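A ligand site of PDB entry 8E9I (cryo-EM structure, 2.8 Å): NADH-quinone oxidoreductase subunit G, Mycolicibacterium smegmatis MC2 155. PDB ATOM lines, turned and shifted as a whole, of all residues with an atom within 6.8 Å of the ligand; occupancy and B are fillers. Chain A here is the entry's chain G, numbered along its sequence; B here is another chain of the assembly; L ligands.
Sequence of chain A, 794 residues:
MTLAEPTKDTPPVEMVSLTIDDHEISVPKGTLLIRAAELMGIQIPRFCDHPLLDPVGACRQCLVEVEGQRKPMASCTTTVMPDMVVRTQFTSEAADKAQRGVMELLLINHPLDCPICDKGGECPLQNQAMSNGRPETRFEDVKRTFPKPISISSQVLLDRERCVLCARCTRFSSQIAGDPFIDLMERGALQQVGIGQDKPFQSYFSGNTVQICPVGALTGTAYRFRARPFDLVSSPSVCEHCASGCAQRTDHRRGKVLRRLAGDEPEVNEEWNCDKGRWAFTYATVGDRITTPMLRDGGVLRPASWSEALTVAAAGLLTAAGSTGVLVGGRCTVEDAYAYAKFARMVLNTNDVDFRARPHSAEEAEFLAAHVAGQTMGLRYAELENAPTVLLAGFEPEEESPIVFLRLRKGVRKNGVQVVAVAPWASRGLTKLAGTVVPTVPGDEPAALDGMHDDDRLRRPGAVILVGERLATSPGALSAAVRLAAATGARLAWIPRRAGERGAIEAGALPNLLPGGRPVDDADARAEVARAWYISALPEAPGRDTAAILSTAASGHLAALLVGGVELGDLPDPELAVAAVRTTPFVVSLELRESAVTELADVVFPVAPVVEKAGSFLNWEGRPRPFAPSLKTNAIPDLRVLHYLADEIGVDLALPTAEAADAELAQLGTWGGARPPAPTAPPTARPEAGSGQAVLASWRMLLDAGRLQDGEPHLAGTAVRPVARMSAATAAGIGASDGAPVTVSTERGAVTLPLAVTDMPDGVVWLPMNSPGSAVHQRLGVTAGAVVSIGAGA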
ATOM      1  N   LEU A 107      18.334  -5.617  22.016  1.00  0.00           N
ATOM      2  CA  LEU A 107      19.025  -5.814  20.754  1.00  0.00           C
ATOM      3  C   LEU A 107      18.952  -4.628  19.801  1.00  0.00           C
ATOM      4  O   LEU A 107      19.715  -4.591  18.839  1.00  0.00           O
ATOM      5  CB  LEU A 107      18.475  -7.050  20.040  1.00  0.00           C
ATOM      6  CG  LEU A 107      18.958  -8.386  20.583  1.00  0.00           C
ATOM      7  CD1 LEU A 107      18.303  -9.517  19.831  1.00  0.00           C
ATOM      8  CD2 LEU A 107      20.461  -8.495  20.497  1.00  0.00           C
ATOM      9  N   HIS A 110      22.173  -2.857  19.674  1.00  0.00           N
ATOM     10  CA  HIS A 110      23.318  -3.741  19.655  1.00  0.00           C
ATOM     11  C   HIS A 110      23.928  -3.796  18.258  1.00  0.00           C
ATOM     12  O   HIS A 110      23.201  -3.852  17.265  1.00  0.00           O
ATOM     13  CB  HIS A 110      22.919  -5.139  20.095  1.00  0.00           C
ATOM     14  CG  HIS A 110      24.043  -5.946  20.639  1.00  0.00           C
ATOM     15  ND1 HIS A 110      24.469  -5.852  21.945  1.00  0.00           N
ATOM     16  CD2 HIS A 110      24.838  -6.877  20.059  1.00  0.00           C
ATOM     17  CE1 HIS A 110      25.471  -6.686  22.144  1.00  0.00           C
ATOM     18  NE2 HIS A 110      25.713  -7.326  21.009  1.00  0.00           N
ATOM     19  N   PRO A 111      25.255  -3.783  18.140  1.00  0.00           N
ATOM     20  CA  PRO A 111      25.868  -3.860  16.810  1.00  0.00           C
ATOM     21  C   PRO A 111      25.603  -5.182  16.120  1.00  0.00           C
ATOM     22  O   PRO A 111      25.478  -6.229  16.759  1.00  0.00           O
ATOM     23  CB  PRO A 111      27.365  -3.688  17.097  1.00  0.00           C
ATOM     24  CG  PRO A 111      27.418  -3.042  18.372  1.00  0.00           C
ATOM     25  CD  PRO A 111      26.277  -3.561  19.167  1.00  0.00           C
ATOM     26  N   LEU A 112      25.571  -5.119  14.802  1.00  0.00           N
ATOM     27  CA  LEU A 112      25.536  -6.317  13.970  1.00  0.00           C
ATOM     28  C   LEU A 112      26.954  -6.877  13.832  1.00  0.00           C
ATOM     29  O   LEU A 112      27.527  -6.966  12.745  1.00  0.00           O
ATOM     30  CB  LEU A 112      24.921  -6.004  12.619  1.00  0.00           C
ATOM     31  CG  LEU A 112      23.406  -6.002  12.555  1.00  0.00           C
ATOM     32  CD1 LEU A 112      22.855  -5.021  13.539  1.00  0.00           C
ATOM     33  CD2 LEU A 112      22.920  -5.677  11.160  1.00  0.00           C
ATOM     34  N   ASP A 113      27.523  -7.247  14.972  1.00  0.00           N
ATOM     35  CA  ASP A 113      28.950  -7.533  15.073  1.00  0.00           C
ATOM     36  C   ASP A 113      29.246  -9.009  15.275  1.00  0.00           C
ATOM     37  O   ASP A 113      30.427  -9.370  15.415  1.00  0.00           O
ATOM     38  CB  ASP A 113      29.564  -6.746  16.225  1.00  0.00           C
ATOM     39  CG  ASP A 113      30.066  -5.388  15.803  1.00  0.00           C
ATOM     40  OD1 ASP A 113      29.786  -4.969  14.669  1.00  0.00           O
ATOM     41  OD2 ASP A 113      30.732  -4.726  16.627  1.00  0.00           O
ATOM     42  N   CYS A 114      28.238  -9.876  15.285  1.00  0.00           N
ATOM     43  CA  CYS A 114      28.478 -11.257  15.689  1.00  0.00           C
ATOM     44  C   CYS A 114      29.606 -11.911  14.918  1.00  0.00           C
ATOM     45  O   CYS A 114      30.456 -12.560  15.551  1.00  0.00           O
ATOM     46  CB  CYS A 114      27.181 -12.064  15.528  1.00  0.00           C
ATOM     47  SG  CYS A 114      25.801 -11.421  16.492  1.00  0.00           S
ATOM     48  N   PRO A 115      29.710 -11.772  13.597  1.00  0.00           N
ATOM     49  CA  PRO A 115      30.859 -12.367  12.906  1.00  0.00           C
ATOM     50  C   PRO A 115      32.199 -11.849  13.391  1.00  0.00           C
ATOM     51  O   PRO A 115      33.171 -12.606  13.432  1.00  0.00           O
ATOM     52  CB  PRO A 115      30.608 -12.002  11.436  1.00  0.00           C
ATOM     53  CG  PRO A 115      29.146 -11.813  11.361  1.00  0.00           C
ATOM     54  CD  PRO A 115      28.779 -11.162  12.646  1.00  0.00           C
ATOM     55  N   ILE A 116      32.275 -10.574  13.787  1.00  0.00           N
ATOM     56  CA  ILE A 116      33.541  -9.999  14.224  1.00  0.00           C
ATOM     57  C   ILE A 116      33.676  -9.940  15.741  1.00  0.00           C
ATOM     58  O   ILE A 116      34.766  -9.655  16.238  1.00  0.00           O
ATOM     59  CB  ILE A 116      33.723  -8.600  13.621  1.00  0.00           C
ATOM     60  CG1 ILE A 116      32.675  -7.622  14.170  1.00  0.00           C
ATOM     61  CG2 ILE A 116      33.608  -8.650  12.115  1.00  0.00           C
ATOM     62  CD1 ILE A 116      33.052  -6.187  13.981  1.00  0.00           C
ATOM     63  N   CYS A 117      32.602 -10.183  16.479  1.00  0.00           N
ATOM     64  CA  CYS A 117      32.678 -10.197  17.935  1.00  0.00           C
ATOM     65  C   CYS A 117      33.338 -11.476  18.419  1.00  0.00           C
ATOM     66  O   CYS A 117      32.935 -12.579  18.026  1.00  0.00           O
ATOM     67  CB  CYS A 117      31.274 -10.078  18.516  1.00  0.00           C
ATOM     68  SG  CYS A 117      31.237 -10.231  20.289  1.00  0.00           S
ATOM     69  N   ASP A 118      34.317 -11.342  19.302  1.00  0.00           N
ATOM     70  CA  ASP A 118      34.975 -12.522  19.854  1.00  0.00           C
ATOM     71  C   ASP A 118      33.997 -13.394  20.612  1.00  0.00           C
ATOM     72  O   ASP A 118      34.135 -14.621  20.631  1.00  0.00           O
ATOM     73  CB  ASP A 118      36.136 -12.112  20.765  1.00  0.00           C
ATOM     74  CG  ASP A 118      37.307 -11.566  19.993  1.00  0.00           C
ATOM     75  OD1 ASP A 118      37.586 -12.090  18.896  1.00  0.00           O
ATOM     76  OD2 ASP A 118      37.949 -10.613  20.472  1.00  0.00           O
ATOM     77  N   LYS A 119      33.006 -12.786  21.257  1.00  0.00           N
ATOM     78  CA  LYS A 119      32.044 -13.559  22.032  1.00  0.00           C
ATOM     79  C   LYS A 119      31.133 -14.403  21.158  1.00  0.00           C
ATOM     80  O   LYS A 119      30.394 -15.239  21.688  1.00  0.00           O
ATOM     81  CB  LYS A 119      31.219 -12.608  22.901  1.00  0.00           C
ATOM     82  CG  LYS A 119      30.385 -13.312  23.945  1.00  0.00           C
ATOM     83  CD  LYS A 119      31.192 -13.860  25.106  1.00  0.00           C
ATOM     84  CE  LYS A 119      31.500 -12.798  26.135  1.00  0.00           C
ATOM     85  NZ  LYS A 119      32.042 -13.410  27.378  1.00  0.00           N
ATOM     86  N   GLY A 120      31.166 -14.236  19.834  1.00  0.00           N
ATOM     87  CA  GLY A 120      30.311 -14.997  18.961  1.00  0.00           C
ATOM     88  C   GLY A 120      30.437 -16.490  19.169  1.00  0.00           C
ATOM     89  O   GLY A 120      31.551 -17.012  19.223  1.00  0.00           O
ATOM     90  N   GLY A 121      29.318 -17.179  19.305  1.00  0.00           N
ATOM     91  CA  GLY A 121      29.324 -18.607  19.579  1.00  0.00           C
ATOM     92  C   GLY A 121      29.251 -18.921  21.042  1.00  0.00           C
ATOM     93  O   GLY A 121      28.624 -19.913  21.440  1.00  0.00           O
ATOM     94  N   GLU A 122      29.892 -18.109  21.872  1.00  0.00           N
ATOM     95  CA  GLU A 122      29.772 -18.239  23.318  1.00  0.00           C
ATOM     96  C   GLU A 122      29.001 -17.094  23.953  1.00  0.00           C
ATOM     97  O   GLU A 122      29.148 -16.870  25.162  1.00  0.00           O
ATOM     98  CB  GLU A 122      31.162 -18.323  23.952  1.00  0.00           C
ATOM     99  N   CYS A 123      28.212 -16.367  23.178  1.00  0.00           N
ATOM    100  CA  CYS A 123      27.564 -15.167  23.695  1.00  0.00           C
ATOM    101  C   CYS A 123      26.251 -15.519  24.374  1.00  0.00           C
ATOM    102  O   CYS A 123      25.367 -16.085  23.719  1.00  0.00           O
ATOM    103  CB  CYS A 123      27.312 -14.190  22.563  1.00  0.00           C
ATOM    104  SG  CYS A 123      26.849 -12.554  23.116  1.00  0.00           S
ATOM    105  N   PRO A 124      26.078 -15.216  25.652  1.00  0.00           N
ATOM    106  CA  PRO A 124      24.755 -15.363  26.255  1.00  0.00           C
ATOM    107  C   PRO A 124      23.704 -14.528  25.571  1.00  0.00           C
ATOM    108  O   PRO A 124      22.536 -14.930  25.504  1.00  0.00           O
ATOM    109  CB  PRO A 124      24.983 -14.935  27.709  1.00  0.00           C
ATOM    110  CG  PRO A 124      26.396 -15.235  27.950  1.00  0.00           C
ATOM    111  CD  PRO A 124      27.108 -14.953  26.676  1.00  0.00           C
ATOM    112  N   LEU A 125      24.059 -13.360  25.043  1.00  0.00           N
ATOM    113  CA  LEU A 125      23.079 -12.549  24.331  1.00  0.00           C
ATOM    114  C   LEU A 125      22.560 -13.279  23.103  1.00  0.00           C
ATOM    115  O   LEU A 125      21.352 -13.330  22.874  1.00  0.00           O
ATOM    116  CB  LEU A 125      23.683 -11.205  23.944  1.00  0.00           C
ATOM    117  CG  LEU A 125      22.794 -10.255  23.150  1.00  0.00           C
ATOM    118  CD1 LEU A 125      21.578  -9.871  23.940  1.00  0.00           C
ATOM    119  CD2 LEU A 125      23.573  -9.027  22.766  1.00  0.00           C
ATOM    120  N   GLN A 126      23.462 -13.841  22.287  1.00  0.00           N
ATOM    121  CA  GLN A 126      23.018 -14.611  21.130  1.00  0.00           C
ATOM    122  C   GLN A 126      22.097 -15.750  21.556  1.00  0.00           C
ATOM    123  O   GLN A 126      21.011 -15.923  20.997  1.00  0.00           O
ATOM    124  CB  GLN A 126      24.214 -15.196  20.388  1.00  0.00           C
ATOM    125  CG  GLN A 126      24.955 -14.250  19.511  1.00  0.00           C
ATOM    126  CD  GLN A 126      26.034 -14.955  18.733  1.00  0.00           C
ATOM    127  OE1 GLN A 126      26.768 -15.766  19.283  1.00  0.00           O
ATOM    128  NE2 GLN A 126      26.134 -14.650  17.450  1.00  0.00           N
ATOM    129  N   ARG A 162      28.252  -2.995  22.160  1.00  0.00           N
ATOM    130  CA  ARG A 162      27.808  -4.323  22.543  1.00  0.00           C
ATOM    131  C   ARG A 162      27.456  -4.405  24.017  1.00  0.00           C
ATOM    132  O   ARG A 162      26.768  -5.350  24.426  1.00  0.00           O
ATOM    133  CB  ARG A 162      28.897  -5.351  22.228  1.00  0.00           C
ATOM    134  CG  ARG A 162      29.295  -5.414  20.778  1.00  0.00           C
ATOM    135  CD  ARG A 162      30.369  -6.442  20.586  1.00  0.00           C
ATOM    136  NE  ARG A 162      31.056  -6.303  19.310  1.00  0.00           N
ATOM    137  CZ  ARG A 162      32.350  -6.533  19.121  1.00  0.00           C
ATOM    138  NH1 ARG A 162      33.143  -6.900  20.110  1.00  0.00           N
ATOM    139  NH2 ARG A 162      32.859  -6.379  17.906  1.00  0.00           N
ATOM    140  N   PRO A 214      28.361 -10.638  29.811  1.00  0.00           N
ATOM    141  CA  PRO A 214      27.487 -11.543  29.067  1.00  0.00           C
ATOM    142  C   PRO A 214      27.478 -11.237  27.576  1.00  0.00           C
ATOM    143  O   PRO A 214      26.661 -11.808  26.845  1.00  0.00           O
ATOM    144  CB  PRO A 214      26.119 -11.290  29.699  1.00  0.00           C
ATOM    145  CG  PRO A 214      26.180  -9.888  30.117  1.00  0.00           C
ATOM    146  CD  PRO A 214      27.581  -9.648  30.583  1.00  0.00           C
ATOM    147  N   VAL A 215      28.358 -10.360  27.127  1.00  0.00           N
ATOM    148  CA  VAL A 215      28.430  -9.966  25.729  1.00  0.00           C
ATOM    149  C   VAL A 215      29.889  -9.717  25.381  1.00  0.00           C
ATOM    150  O   VAL A 215      30.779  -9.900  26.204  1.00  0.00           O
ATOM    151  CB  VAL A 215      27.578  -8.714  25.432  1.00  0.00           C
ATOM    152  CG1 VAL A 215      26.123  -9.051  25.521  1.00  0.00           C
ATOM    153  CG2 VAL A 215      27.922  -7.608  26.386  1.00  0.00           C
ATOM    154  N   GLY A 216      30.125  -9.284  24.145  1.00  0.00           N
ATOM    155  CA  GLY A 216      31.470  -9.048  23.678  1.00  0.00           C
ATOM    156  C   GLY A 216      31.991  -7.671  24.031  1.00  0.00           C
ATOM    157  O   GLY A 216      32.993  -7.226  23.462  1.00  0.00           O
ATOM    158  N   ALA A 217      31.329  -6.989  24.958  1.00  0.00           N
ATOM    159  CA  ALA A 217      31.740  -5.637  25.322  1.00  0.00           C
ATOM    160  C   ALA A 217      33.163  -5.632  25.858  1.00  0.00           C
ATOM    161  O   ALA A 217      34.006  -4.855  25.394  1.00  0.00           O
ATOM    162  CB  ALA A 217      30.765  -5.061  26.337  1.00  0.00           C
ATOM    163  N   ARG A 228      37.399 -18.966  17.461  1.00  0.00           N
ATOM    164  CA  ARG A 228      36.007 -19.132  17.810  1.00  0.00           C
ATOM    165  C   ARG A 228      35.827 -20.387  18.640  1.00  0.00           C
ATOM    166  O   ARG A 228      36.652 -21.296  18.591  1.00  0.00           O
ATOM    167  CB  ARG A 228      35.131 -19.219  16.555  1.00  0.00           C
ATOM    168  CG  ARG A 228      35.481 -18.226  15.449  1.00  0.00           C
ATOM    169  CD  ARG A 228      35.574 -16.797  15.952  1.00  0.00           C
ATOM    170  NE  ARG A 228      34.298 -16.253  16.386  1.00  0.00           N
ATOM    171  CZ  ARG A 228      33.519 -15.492  15.647  1.00  0.00           C
ATOM    172  NH1 ARG A 228      33.801 -15.227  14.390  1.00  0.00           N
ATOM    173  NH2 ARG A 228      32.418 -14.971  16.191  1.00  0.00           N
ATOM    174  N   MET B 354      19.454  -7.277  13.439  1.00  0.00           N
ATOM    175  CA  MET B 354      20.278  -7.875  14.478  1.00  0.00           C
ATOM    176  C   MET B 354      19.776  -9.265  14.853  1.00  0.00           C
ATOM    177  O   MET B 354      20.568 -10.212  14.962  1.00  0.00           O
ATOM    178  CB  MET B 354      20.320  -6.989  15.714  1.00  0.00           C
ATOM    179  CG  MET B 354      21.272  -7.485  16.775  1.00  0.00           C
ATOM    180  SD  MET B 354      22.971  -7.426  16.221  1.00  0.00           S
ATOM    181  CE  MET B 354      23.730  -8.667  17.266  1.00  0.00           C
ATOM    182  N   LEU B 357      20.812 -11.494  12.184  1.00  0.00           N
ATOM    183  CA  LEU B 357      22.213 -11.881  12.279  1.00  0.00           C
ATOM    184  C   LEU B 357      22.415 -12.957  13.326  1.00  0.00           C
ATOM    185  O   LEU B 357      23.135 -13.930  13.097  1.00  0.00           O
ATOM    186  CB  LEU B 357      23.069 -10.652  12.612  1.00  0.00           C
ATOM    187  CG  LEU B 357      24.574 -10.881  12.699  1.00  0.00           C
ATOM    188  CD1 LEU B 357      25.100 -11.508  11.421  1.00  0.00           C
ATOM    189  CD2 LEU B 357      25.273  -9.564  12.962  1.00  0.00           C
ATOM    190  N   ILE B 358      21.782 -12.802  14.487  1.00  0.00           N
ATOM    191  CA  ILE B 358      21.952 -13.790  15.550  1.00  0.00           C
ATOM    192  C   ILE B 358      21.425 -15.138  15.081  1.00  0.00           C
ATOM    193  O   ILE B 358      22.037 -16.187  15.332  1.00  0.00           O
ATOM    194  CB  ILE B 358      21.242 -13.334  16.837  1.00  0.00           C
ATOM    195  CG1 ILE B 358      22.001 -12.165  17.449  1.00  0.00           C
ATOM    196  CG2 ILE B 358      21.143 -14.479  17.815  1.00  0.00           C
ATOM    197  CD1 ILE B 358      21.278 -11.503  18.599  1.00  0.00           C
ATOM    198  N   PHE B 361      23.793 -16.696  12.537  1.00  0.00           N
ATOM    199  CA  PHE B 361      25.008 -17.139  13.219  1.00  0.00           C
ATOM    200  C   PHE B 361      24.767 -18.427  13.996  1.00  0.00           C
ATOM    201  O   PHE B 361      25.532 -19.389  13.890  1.00  0.00           O
ATOM    202  CB  PHE B 361      25.490 -16.012  14.141  1.00  0.00           C
ATOM    203  CG  PHE B 361      26.861 -16.205  14.696  1.00  0.00           C
ATOM    204  CD1 PHE B 361      27.115 -17.180  15.636  1.00  0.00           C
ATOM    205  CD2 PHE B 361      27.895 -15.391  14.291  1.00  0.00           C
ATOM    206  CE1 PHE B 361      28.372 -17.339  16.152  1.00  0.00           C
ATOM    207  CE2 PHE B 361      29.153 -15.551  14.807  1.00  0.00           C
ATOM    208  CZ  PHE B 361      29.386 -16.525  15.737  1.00  0.00           C
HETATM  209 FE1  LIG L   1      26.770 -10.978  18.473  1.00  0.00          FE
HETATM  210 FE2  LIG L   1      26.971 -11.432  21.159  1.00  0.00          FE
HETATM  211 FE3  LIG L   1      26.675  -8.886  20.224  1.00  0.00          FE
HETATM  212 FE4  LIG L   1      29.026 -10.224  19.830  1.00  0.00          FE
HETATM  213  S1  LIG L   1      28.136  -9.600  21.824  1.00  0.00           S
HETATM  214  S2  LIG L   1      27.868  -8.993  18.294  1.00  0.00           S
HETATM  215  S3  LIG L   1      28.256 -12.347  19.514  1.00  0.00           S
HETATM  216  S4  LIG L   1      25.173 -10.590  20.052  1.00  0.00           S
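N of Leu 125 sits close to SG of Cys 123 (3.5 Å). The side-chain sulfur (SG) of Cys 114 sits close to the side-chain amide nitrogen (NE2) of Gln 126. The backbone carbonyl oxygen of Cys 117 lies within hydrogen-bond range of the guanidinium group of Arg 228 (3.1 Å). The backbone NH (N) of Gly 121 is in hydrogen-bond range of the side-chain amide oxygen (OE1) of Gln 126, 2.9 Å away. The backbone carbonyl oxygen (O) of Gly 216 sits at hydrogen-bond distance from the guanidinium group (NH1) of Arg 162 (3.4 Å). A ring nitrogen (ND1) of His 110 sits close to the backbone carbonyl oxygen (O) of Arg 162 (3.4 Å). The backbone NH (N) of Leu 112 sits close to the side-chain sulfur (SD) of Met 354 of chain B, 3.8 Å away. The backbone carbonyl oxygen of Cys 114 lies within hydrogen-bond range of the guanidinium group of Arg 228, 3.2 Å away.
SG of Cys 114 is bound to FE1 of the ligand (2.2 Å). The side-chain sulfur (SG) of Cys 123 binds an iron atom (FE2) of the ligand (2.3 Å). N of Gly 120 sits close to S3 of the ligand (3.5 Å). A sulfur (S2) of the ligand sits close to the backbone NH of Cys 114 (3.2 Å). S3 of the ligand sits close to OE1 of Gln 126 (3.7 Å). An iron atom (FE3) of the ligand is bound by a ring nitrogen (NE2) of His 110, at 2.0 Å. The backbone NH (N) of Asp 113 lies close to a sulfur (S2) of the ligand, 3.8 Å away. SG of Cys 117 binds FE4 of the ligand (2.3 Å). S1 of the ligand lies close to N of Gly 216 (3.1 Å).
Merely in contact with the ligand: Leu 125, Met 354 of chain B, Val 215, Lys 119 and Pro 111. Hydrophobic or aromatic side chains that line the ligand: His 110, Leu 125, Val 215 and Met 354 of chain B. 13 residues have an atom within 4 Å of the ligand: His 110, Pro 111, Asp 113, Cys 114, Cys 117, Lys 119, Gly 120, Cys 123, Leu 125, Gln 126, Val 215, Gly 216 and Met 354 of chain B. Along chain A the residues within 4 Å of the ligand span positions 110 to 216.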
